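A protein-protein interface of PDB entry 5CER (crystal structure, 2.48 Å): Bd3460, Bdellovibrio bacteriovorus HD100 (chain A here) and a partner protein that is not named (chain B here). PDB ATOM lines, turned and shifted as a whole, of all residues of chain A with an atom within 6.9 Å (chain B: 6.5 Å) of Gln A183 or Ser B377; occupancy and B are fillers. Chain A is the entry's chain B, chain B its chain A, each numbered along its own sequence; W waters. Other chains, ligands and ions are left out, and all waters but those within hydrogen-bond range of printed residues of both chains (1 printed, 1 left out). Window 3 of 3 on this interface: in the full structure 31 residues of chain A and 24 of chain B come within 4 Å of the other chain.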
ATOM      1  N   ALA A 145      -5.189  22.627  26.223  1.00  0.00           N
ATOM      2  CA  ALA A 145      -4.557  22.174  24.981  1.00  0.00           C
ATOM      3  C   ALA A 145      -5.256  20.960  24.396  1.00  0.00           C
ATOM      4  O   ALA A 145      -5.397  20.850  23.158  1.00  0.00           O
ATOM      5  CB  ALA A 145      -3.061  21.870  25.185  1.00  0.00           C
ATOM      6  N   ALA A 177      -1.799  18.449  22.748  1.00  0.00           N
ATOM      7  CA  ALA A 177      -2.734  19.005  21.759  1.00  0.00           C
ATOM      8  C   ALA A 177      -2.748  18.148  20.498  1.00  0.00           C
ATOM      9  O   ALA A 177      -3.825  17.859  19.946  1.00  0.00           O
ATOM     10  CB  ALA A 177      -2.377  20.458  21.414  1.00  0.00           C
ATOM     11  N   LYS A 178      -1.560  17.759  20.046  1.00  0.00           N
ATOM     12  CA  LYS A 178      -1.428  17.005  18.801  1.00  0.00           C
ATOM     13  C   LYS A 178      -1.954  15.592  18.989  1.00  0.00           C
ATOM     14  O   LYS A 178      -2.687  15.086  18.144  1.00  0.00           O
ATOM     15  CB  LYS A 178       0.024  16.963  18.302  1.00  0.00           C
ATOM     16  CG  LYS A 178       0.616  18.346  18.015  1.00  0.00           C
ATOM     17  CD  LYS A 178       2.085  18.322  17.642  1.00  0.00           C
ATOM     18  CE  LYS A 178       2.573  19.504  16.831  1.00  0.00           C
ATOM     19  NZ  LYS A 178       3.956  19.182  16.345  1.00  0.00           N
ATOM     20  N   ALA A 180      -4.201  14.730  21.052  1.00  0.00           N
ATOM     21  CA  ALA A 180      -5.645  14.857  21.150  1.00  0.00           C
ATOM     22  C   ALA A 180      -6.347  15.262  19.856  1.00  0.00           C
ATOM     23  O   ALA A 180      -7.574  15.319  19.816  1.00  0.00           O
ATOM     24  CB  ALA A 180      -5.985  15.858  22.243  1.00  0.00           C
ATOM     25  N   SER A 181      -5.583  15.554  18.796  1.00  0.00           N
ATOM     26  CA  SER A 181      -6.100  16.056  17.511  1.00  0.00           C
ATOM     27  C   SER A 181      -6.824  17.380  17.600  1.00  0.00           C
ATOM     28  O   SER A 181      -7.734  17.642  16.811  1.00  0.00           O
ATOM     29  CB  SER A 181      -7.009  15.027  16.836  1.00  0.00           C
ATOM     30  OG  SER A 181      -6.406  13.740  16.888  1.00  0.00           O
ATOM     31  N   ASN A 182      -6.441  18.213  18.567  1.00  0.00           N
ATOM     32  CA  ASN A 182      -6.965  19.567  18.667  1.00  0.00           C
ATOM     33  C   ASN A 182      -6.089  20.473  17.798  1.00  0.00           C
ATOM     34  O   ASN A 182      -5.075  21.039  18.268  1.00  0.00           O
ATOM     35  CB  ASN A 182      -6.973  20.025  20.128  1.00  0.00           C
ATOM     36  CG  ASN A 182      -7.766  21.319  20.349  1.00  0.00           C
ATOM     37  OD1 ASN A 182      -7.907  22.150  19.448  1.00  0.00           O
ATOM     38  ND2 ASN A 182      -8.285  21.483  21.561  1.00  0.00           N
ATOM     39  N   GLN A 183      -6.470  20.585  16.532  1.00  0.00           N
ATOM     40  CA  GLN A 183      -5.661  21.294  15.545  1.00  0.00           C
ATOM     41  C   GLN A 183      -5.618  22.769  15.913  1.00  0.00           C
ATOM     42  O   GLN A 183      -4.599  23.415  15.710  1.00  0.00           O
ATOM     43  CB  GLN A 183      -6.208  21.088  14.115  1.00  0.00           C
ATOM     44  CG  GLN A 183      -6.418  19.630  13.702  1.00  0.00           C
ATOM     45  CD  GLN A 183      -7.230  19.475  12.425  1.00  0.00           C
ATOM     46  OE1 GLN A 183      -6.856  19.981  11.379  1.00  0.00           O
ATOM     47  NE2 GLN A 183      -8.336  18.757  12.506  1.00  0.00           N
ATOM     48  N   ASP A 184      -6.699  23.283  16.500  1.00  0.00           N
ATOM     49  CA  ASP A 184      -6.818  24.711  16.833  1.00  0.00           C
ATOM     50  C   ASP A 184      -5.833  25.135  17.924  1.00  0.00           C
ATOM     51  O   ASP A 184      -5.147  26.142  17.769  1.00  0.00           O
ATOM     52  CB  ASP A 184      -8.259  25.108  17.249  1.00  0.00           C
ATOM     53  CG  ASP A 184      -9.291  24.997  16.106  1.00  0.00           C
ATOM     54  OD1 ASP A 184      -8.920  24.983  14.919  1.00  0.00           O
ATOM     55  OD2 ASP A 184     -10.514  24.951  16.399  1.00  0.00           O
ATOM     56  N   THR A 185      -5.778  24.396  19.027  1.00  0.00           N
ATOM     57  CA  THR A 185      -4.849  24.715  20.114  1.00  0.00           C
ATOM     58  C   THR A 185      -3.419  24.368  19.703  1.00  0.00           C
ATOM     59  O   THR A 185      -2.493  25.082  20.072  1.00  0.00           O
ATOM     60  CB  THR A 185      -5.191  23.991  21.426  1.00  0.00           C
ATOM     61  OG1 THR A 185      -5.211  22.585  21.196  1.00  0.00           O
ATOM     62  CG2 THR A 185      -6.523  24.446  21.947  1.00  0.00           C
ATOM     63  N   ALA A 186      -3.253  23.304  18.913  1.00  0.00           N
ATOM     64  CA  ALA A 186      -1.946  22.933  18.392  1.00  0.00           C
ATOM     65  C   ALA A 186      -1.349  24.081  17.604  1.00  0.00           C
ATOM     66  O   ALA A 186      -0.199  24.494  17.861  1.00  0.00           O
ATOM     67  CB  ALA A 186      -2.038  21.698  17.527  1.00  0.00           C
ATOM     68  N   LYS A 187      -2.129  24.606  16.656  1.00  0.00           N
ATOM     69  CA  LYS A 187      -1.712  25.797  15.873  1.00  0.00           C
ATOM     70  C   LYS A 187      -1.357  26.970  16.777  1.00  0.00           C
ATOM     71  O   LYS A 187      -0.270  27.489  16.654  1.00  0.00           O
ATOM     72  CB  LYS A 187      -2.700  26.171  14.709  1.00  0.00           C
ATOM     73  CG  LYS A 187      -2.253  25.647  13.329  1.00  0.00           C
ATOM     74  CD  LYS A 187      -3.320  25.551  12.197  1.00  0.00           C
ATOM     75  CE  LYS A 187      -4.580  24.790  12.625  1.00  0.00           C
ATOM     76  NZ  LYS A 187      -5.554  24.482  11.529  1.00  0.00           N
ATOM     77  N   ALA A 188      -2.239  27.331  17.711  1.00  0.00           N
ATOM     78  CA  ALA A 188      -2.010  28.459  18.646  1.00  0.00           C
ATOM     79  C   ALA A 188      -0.740  28.267  19.469  1.00  0.00           C
ATOM     80  O   ALA A 188       0.012  29.199  19.682  1.00  0.00           O
ATOM     81  CB  ALA A 188      -3.217  28.658  19.560  1.00  0.00           C
ATOM     82  N   SER A 190       1.903  26.166  18.749  1.00  0.00           N
ATOM     83  CA  SER A 190       3.088  26.024  17.909  1.00  0.00           C
ATOM     84  C   SER A 190       3.501  27.319  17.208  1.00  0.00           C
ATOM     85  O   SER A 190       4.641  27.412  16.739  1.00  0.00           O
ATOM     86  CB  SER A 190       2.889  24.910  16.893  1.00  0.00           C
ATOM     87  OG  SER A 190       1.866  25.242  15.982  1.00  0.00           O
ATOM     88  N   THR B 336     -19.395  21.388  14.372  1.00  0.00           N
ATOM     89  CA  THR B 336     -17.987  21.242  14.069  1.00  0.00           C
ATOM     90  C   THR B 336     -17.749  21.617  12.629  1.00  0.00           C
ATOM     91  O   THR B 336     -18.688  21.738  11.836  1.00  0.00           O
ATOM     92  CB  THR B 336     -17.551  19.775  14.231  1.00  0.00           C
ATOM     93  OG1 THR B 336     -18.007  18.983  13.118  1.00  0.00           O
ATOM     94  CG2 THR B 336     -18.103  19.177  15.518  1.00  0.00           C
ATOM     95  N   LYS B 337     -16.480  21.748  12.259  1.00  0.00           N
ATOM     96  CA  LYS B 337     -16.130  22.043  10.868  1.00  0.00           C
ATOM     97  C   LYS B 337     -16.539  20.951   9.869  1.00  0.00           C
ATOM     98  O   LYS B 337     -16.517  21.200   8.679  1.00  0.00           O
ATOM     99  CB  LYS B 337     -14.636  22.406  10.748  1.00  0.00           C
ATOM    100  CG  LYS B 337     -14.304  23.707  11.456  1.00  0.00           C
ATOM    101  CD  LYS B 337     -12.920  24.237  11.115  1.00  0.00           C
ATOM    102  CE  LYS B 337     -12.511  25.446  11.966  1.00  0.00           C
ATOM    103  NZ  LYS B 337     -12.126  25.039  13.366  1.00  0.00           N
ATOM    104  N   GLU B 338     -16.840  19.736  10.331  1.00  0.00           N
ATOM    105  CA  GLU B 338     -17.377  18.675   9.471  1.00  0.00           C
ATOM    106  C   GLU B 338     -18.908  18.556   9.551  1.00  0.00           C
ATOM    107  O   GLU B 338     -19.456  17.548   9.109  1.00  0.00           O
ATOM    108  CB  GLU B 338     -16.754  17.344   9.827  1.00  0.00           C
ATOM    109  CG  GLU B 338     -15.276  17.273   9.503  1.00  0.00           C
ATOM    110  CD  GLU B 338     -14.633  16.005  10.000  1.00  0.00           C
ATOM    111  OE1 GLU B 338     -15.374  15.041  10.318  1.00  0.00           O
ATOM    112  OE2 GLU B 338     -13.392  15.960  10.090  1.00  0.00           O
ATOM    113  N   LEU B 372     -14.644  14.430  20.831  1.00  0.00           N
ATOM    114  CA  LEU B 372     -15.473  14.261  19.639  1.00  0.00           C
ATOM    115  C   LEU B 372     -15.351  15.472  18.735  1.00  0.00           C
ATOM    116  O   LEU B 372     -15.211  15.333  17.512  1.00  0.00           O
ATOM    117  CB  LEU B 372     -16.936  14.132  20.020  1.00  0.00           C
ATOM    118  CG  LEU B 372     -17.449  12.890  20.734  1.00  0.00           C
ATOM    119  CD1 LEU B 372     -18.931  12.943  21.021  1.00  0.00           C
ATOM    120  CD2 LEU B 372     -17.133  11.599  19.960  1.00  0.00           C
ATOM    121  N   ILE B 373     -15.350  16.664  19.324  1.00  0.00           N
ATOM    122  CA  ILE B 373     -15.123  17.890  18.533  1.00  0.00           C
ATOM    123  C   ILE B 373     -13.732  17.889  17.834  1.00  0.00           C
ATOM    124  O   ILE B 373     -13.654  18.174  16.637  1.00  0.00           O
ATOM    125  CB  ILE B 373     -15.375  19.162  19.369  1.00  0.00           C
ATOM    126  CG1 ILE B 373     -16.885  19.250  19.666  1.00  0.00           C
ATOM    127  CG2 ILE B 373     -14.903  20.409  18.649  1.00  0.00           C
ATOM    128  CD1 ILE B 373     -17.237  20.285  20.735  1.00  0.00           C
ATOM    129  N   ASN B 374     -12.676  17.570  18.572  1.00  0.00           N
ATOM    130  CA  ASN B 374     -11.348  17.477  18.020  1.00  0.00           C
ATOM    131  C   ASN B 374     -11.279  16.618  16.778  1.00  0.00           C
ATOM    132  O   ASN B 374     -10.690  17.039  15.781  1.00  0.00           O
ATOM    133  CB  ASN B 374     -10.371  16.924  19.054  1.00  0.00           C
ATOM    134  CG  ASN B 374     -10.107  17.888  20.208  1.00  0.00           C
ATOM    135  OD1 ASN B 374     -10.226  19.117  20.060  1.00  0.00           O
ATOM    136  ND2 ASN B 374      -9.629  17.347  21.321  1.00  0.00           N
ATOM    137  N   LYS B 375     -11.863  15.428  16.861  1.00  0.00           N
ATOM    138  CA  LYS B 375     -11.873  14.465  15.774  1.00  0.00           C
ATOM    139  C   LYS B 375     -12.739  14.872  14.591  1.00  0.00           C
ATOM    140  O   LYS B 375     -12.613  14.310  13.518  1.00  0.00           O
ATOM    141  CB  LYS B 375     -12.391  13.115  16.277  1.00  0.00           C
ATOM    142  CG  LYS B 375     -11.476  12.395  17.231  1.00  0.00           C
ATOM    143  CD  LYS B 375     -10.192  11.948  16.527  1.00  0.00           C
ATOM    144  CE  LYS B 375      -9.504  10.801  17.242  1.00  0.00           C
ATOM    145  NZ  LYS B 375      -8.578  10.105  16.299  1.00  0.00           N
ATOM    146  N   ARG B 376     -13.606  15.842  14.786  1.00  0.00           N
ATOM    147  CA  ARG B 376     -14.361  16.435  13.684  1.00  0.00           C
ATOM    148  C   ARG B 376     -13.848  17.845  13.261  1.00  0.00           C
ATOM    149  O   ARG B 376     -14.606  18.711  12.781  1.00  0.00           O
ATOM    150  CB  ARG B 376     -15.839  16.403  14.069  1.00  0.00           C
ATOM    151  CG  ARG B 376     -16.375  15.000  13.944  1.00  0.00           C
ATOM    152  CD  ARG B 376     -17.493  14.722  14.888  1.00  0.00           C
ATOM    153  NE  ARG B 376     -17.737  13.275  14.884  1.00  0.00           N
ATOM    154  CZ  ARG B 376     -17.081  12.373  15.632  1.00  0.00           C
ATOM    155  NH1 ARG B 376     -16.125  12.738  16.489  1.00  0.00           N
ATOM    156  NH2 ARG B 376     -17.380  11.079  15.529  1.00  0.00           N
ATOM    157  N   SER B 377     -12.532  18.036  13.417  1.00  0.00           N
ATOM    158  CA  SER B 377     -11.822  19.232  12.941  1.00  0.00           C
ATOM    159  C   SER B 377     -12.170  20.527  13.669  1.00  0.00           C
ATOM    160  O   SER B 377     -11.975  21.617  13.153  1.00  0.00           O
ATOM    161  CB  SER B 377     -11.943  19.381  11.412  1.00  0.00           C
ATOM    162  OG  SER B 377     -11.201  18.366  10.742  1.00  0.00           O
ATOM    163  N   GLY B 378     -12.607  20.400  14.917  1.00  0.00           N
ATOM    164  CA  GLY B 378     -12.770  21.543  15.791  1.00  0.00           C
ATOM    165  C   GLY B 378     -14.153  22.150  15.740  1.00  0.00           C
ATOM    166  O   GLY B 378     -14.983  21.766  14.933  1.00  0.00           O
ATOM    167  N   PRO B 379     -14.404  23.110  16.612  1.00  0.00           N
ATOM    168  CA  PRO B 379     -15.734  23.640  16.741  1.00  0.00           C
ATOM    169  C   PRO B 379     -16.082  24.596  15.624  1.00  0.00           C
ATOM    170  O   PRO B 379     -15.199  25.242  15.058  1.00  0.00           O
ATOM    171  CB  PRO B 379     -15.669  24.377  18.078  1.00  0.00           C
ATOM    172  CG  PRO B 379     -14.246  24.757  18.252  1.00  0.00           C
ATOM    173  CD  PRO B 379     -13.462  23.668  17.599  1.00  0.00           C
HETATM  174  O   HOH W   1     -10.682  21.247  18.512  1.00  0.00           O
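Among the printed residues, merely in contact across the chains: Asp A184 with Pro B379 (3.4 Å).
Gln A183 touches just one residue of chain B: Ser B377 (3.4 Å). Of the printed residues of chain A, Ser B377 touches Gln A183 (3.4 Å). Printed residues of chain B within 4 Å of Asn A182: Asn B374 (3.3 Å). Of the printed residues of chain B, Asp A184 touches Lys B337 (3.4 Å) and Pro B379 (3.4 Å). Of the printed residues of chain B, Ala A180 touches Asn B374 (3.3 Å). Of the printed residues of chain A, Pro B379 touches Asp A184 (3.4 Å). The nearest residue of chain B that does not touch Gln A183 is Asn B374 (4.4 Å). The nearest printed residue of chain B that does not touch Ala A180 is Lys B375 (5.2 Å).
The side-chain carboxylate (OD2) of Asp A184 is in salt-bridge range of the side-chain amino group (NZ) of Lys B337 (3.4 Å). ND2 of Asn B374 lies within hydrogen-bond range of O of Ala A180 (3.3 Å). OD1 of Asn B374 lies close to ND2 of Asn A182. OG of Ser B377 is in hydrogen-bond range of NE2 of Gln A183. The backbone carbonyl oxygen of Ser A181 sits close to the backbone carbonyl oxygen of Asn B374 (3.2 Å).
The backbone NH of Lys B337 sits at hydrogen-bond distance from the backbone carbonyl oxygen of Gly B378, at 3.1 Å. The side-chain carboxylate of Glu B338 sits at hydrogen-bond distance from the side-chain hydroxyl of Ser B377. The side-chain amide nitrogen (ND2) of Asn A182 is in hydrogen-bond range of the backbone carbonyl oxygen (O) of Ala A145 (3.4 Å). The backbone NH (N) of Asn A182 lies within hydrogen-bond range of the backbone carbonyl oxygen (O) of Ala A177 (3.0 Å). The side-chain amide oxygen (OD1) of Asn A182 lies close to the backbone NH (N) of Asp A184 (3.4 Å). N of Thr A185 sits at hydrogen-bond distance from OD1 of Asn A182, 3.1 Å away.
Along chain A the printed residues that touch a printed residue of chain B span positions 180 to 184. Printed residues of chain B that touch a printed residue of chain A: Lys B337, Asn B374, Ser B377 and Pro B379. Along chain B the printed residues that touch a printed residue of chain A span positions 337 to 379.
Water W1 bridges OD1 of Asn B374 (2.7 Å) and OD1 of Asn A182 (3.1 Å).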
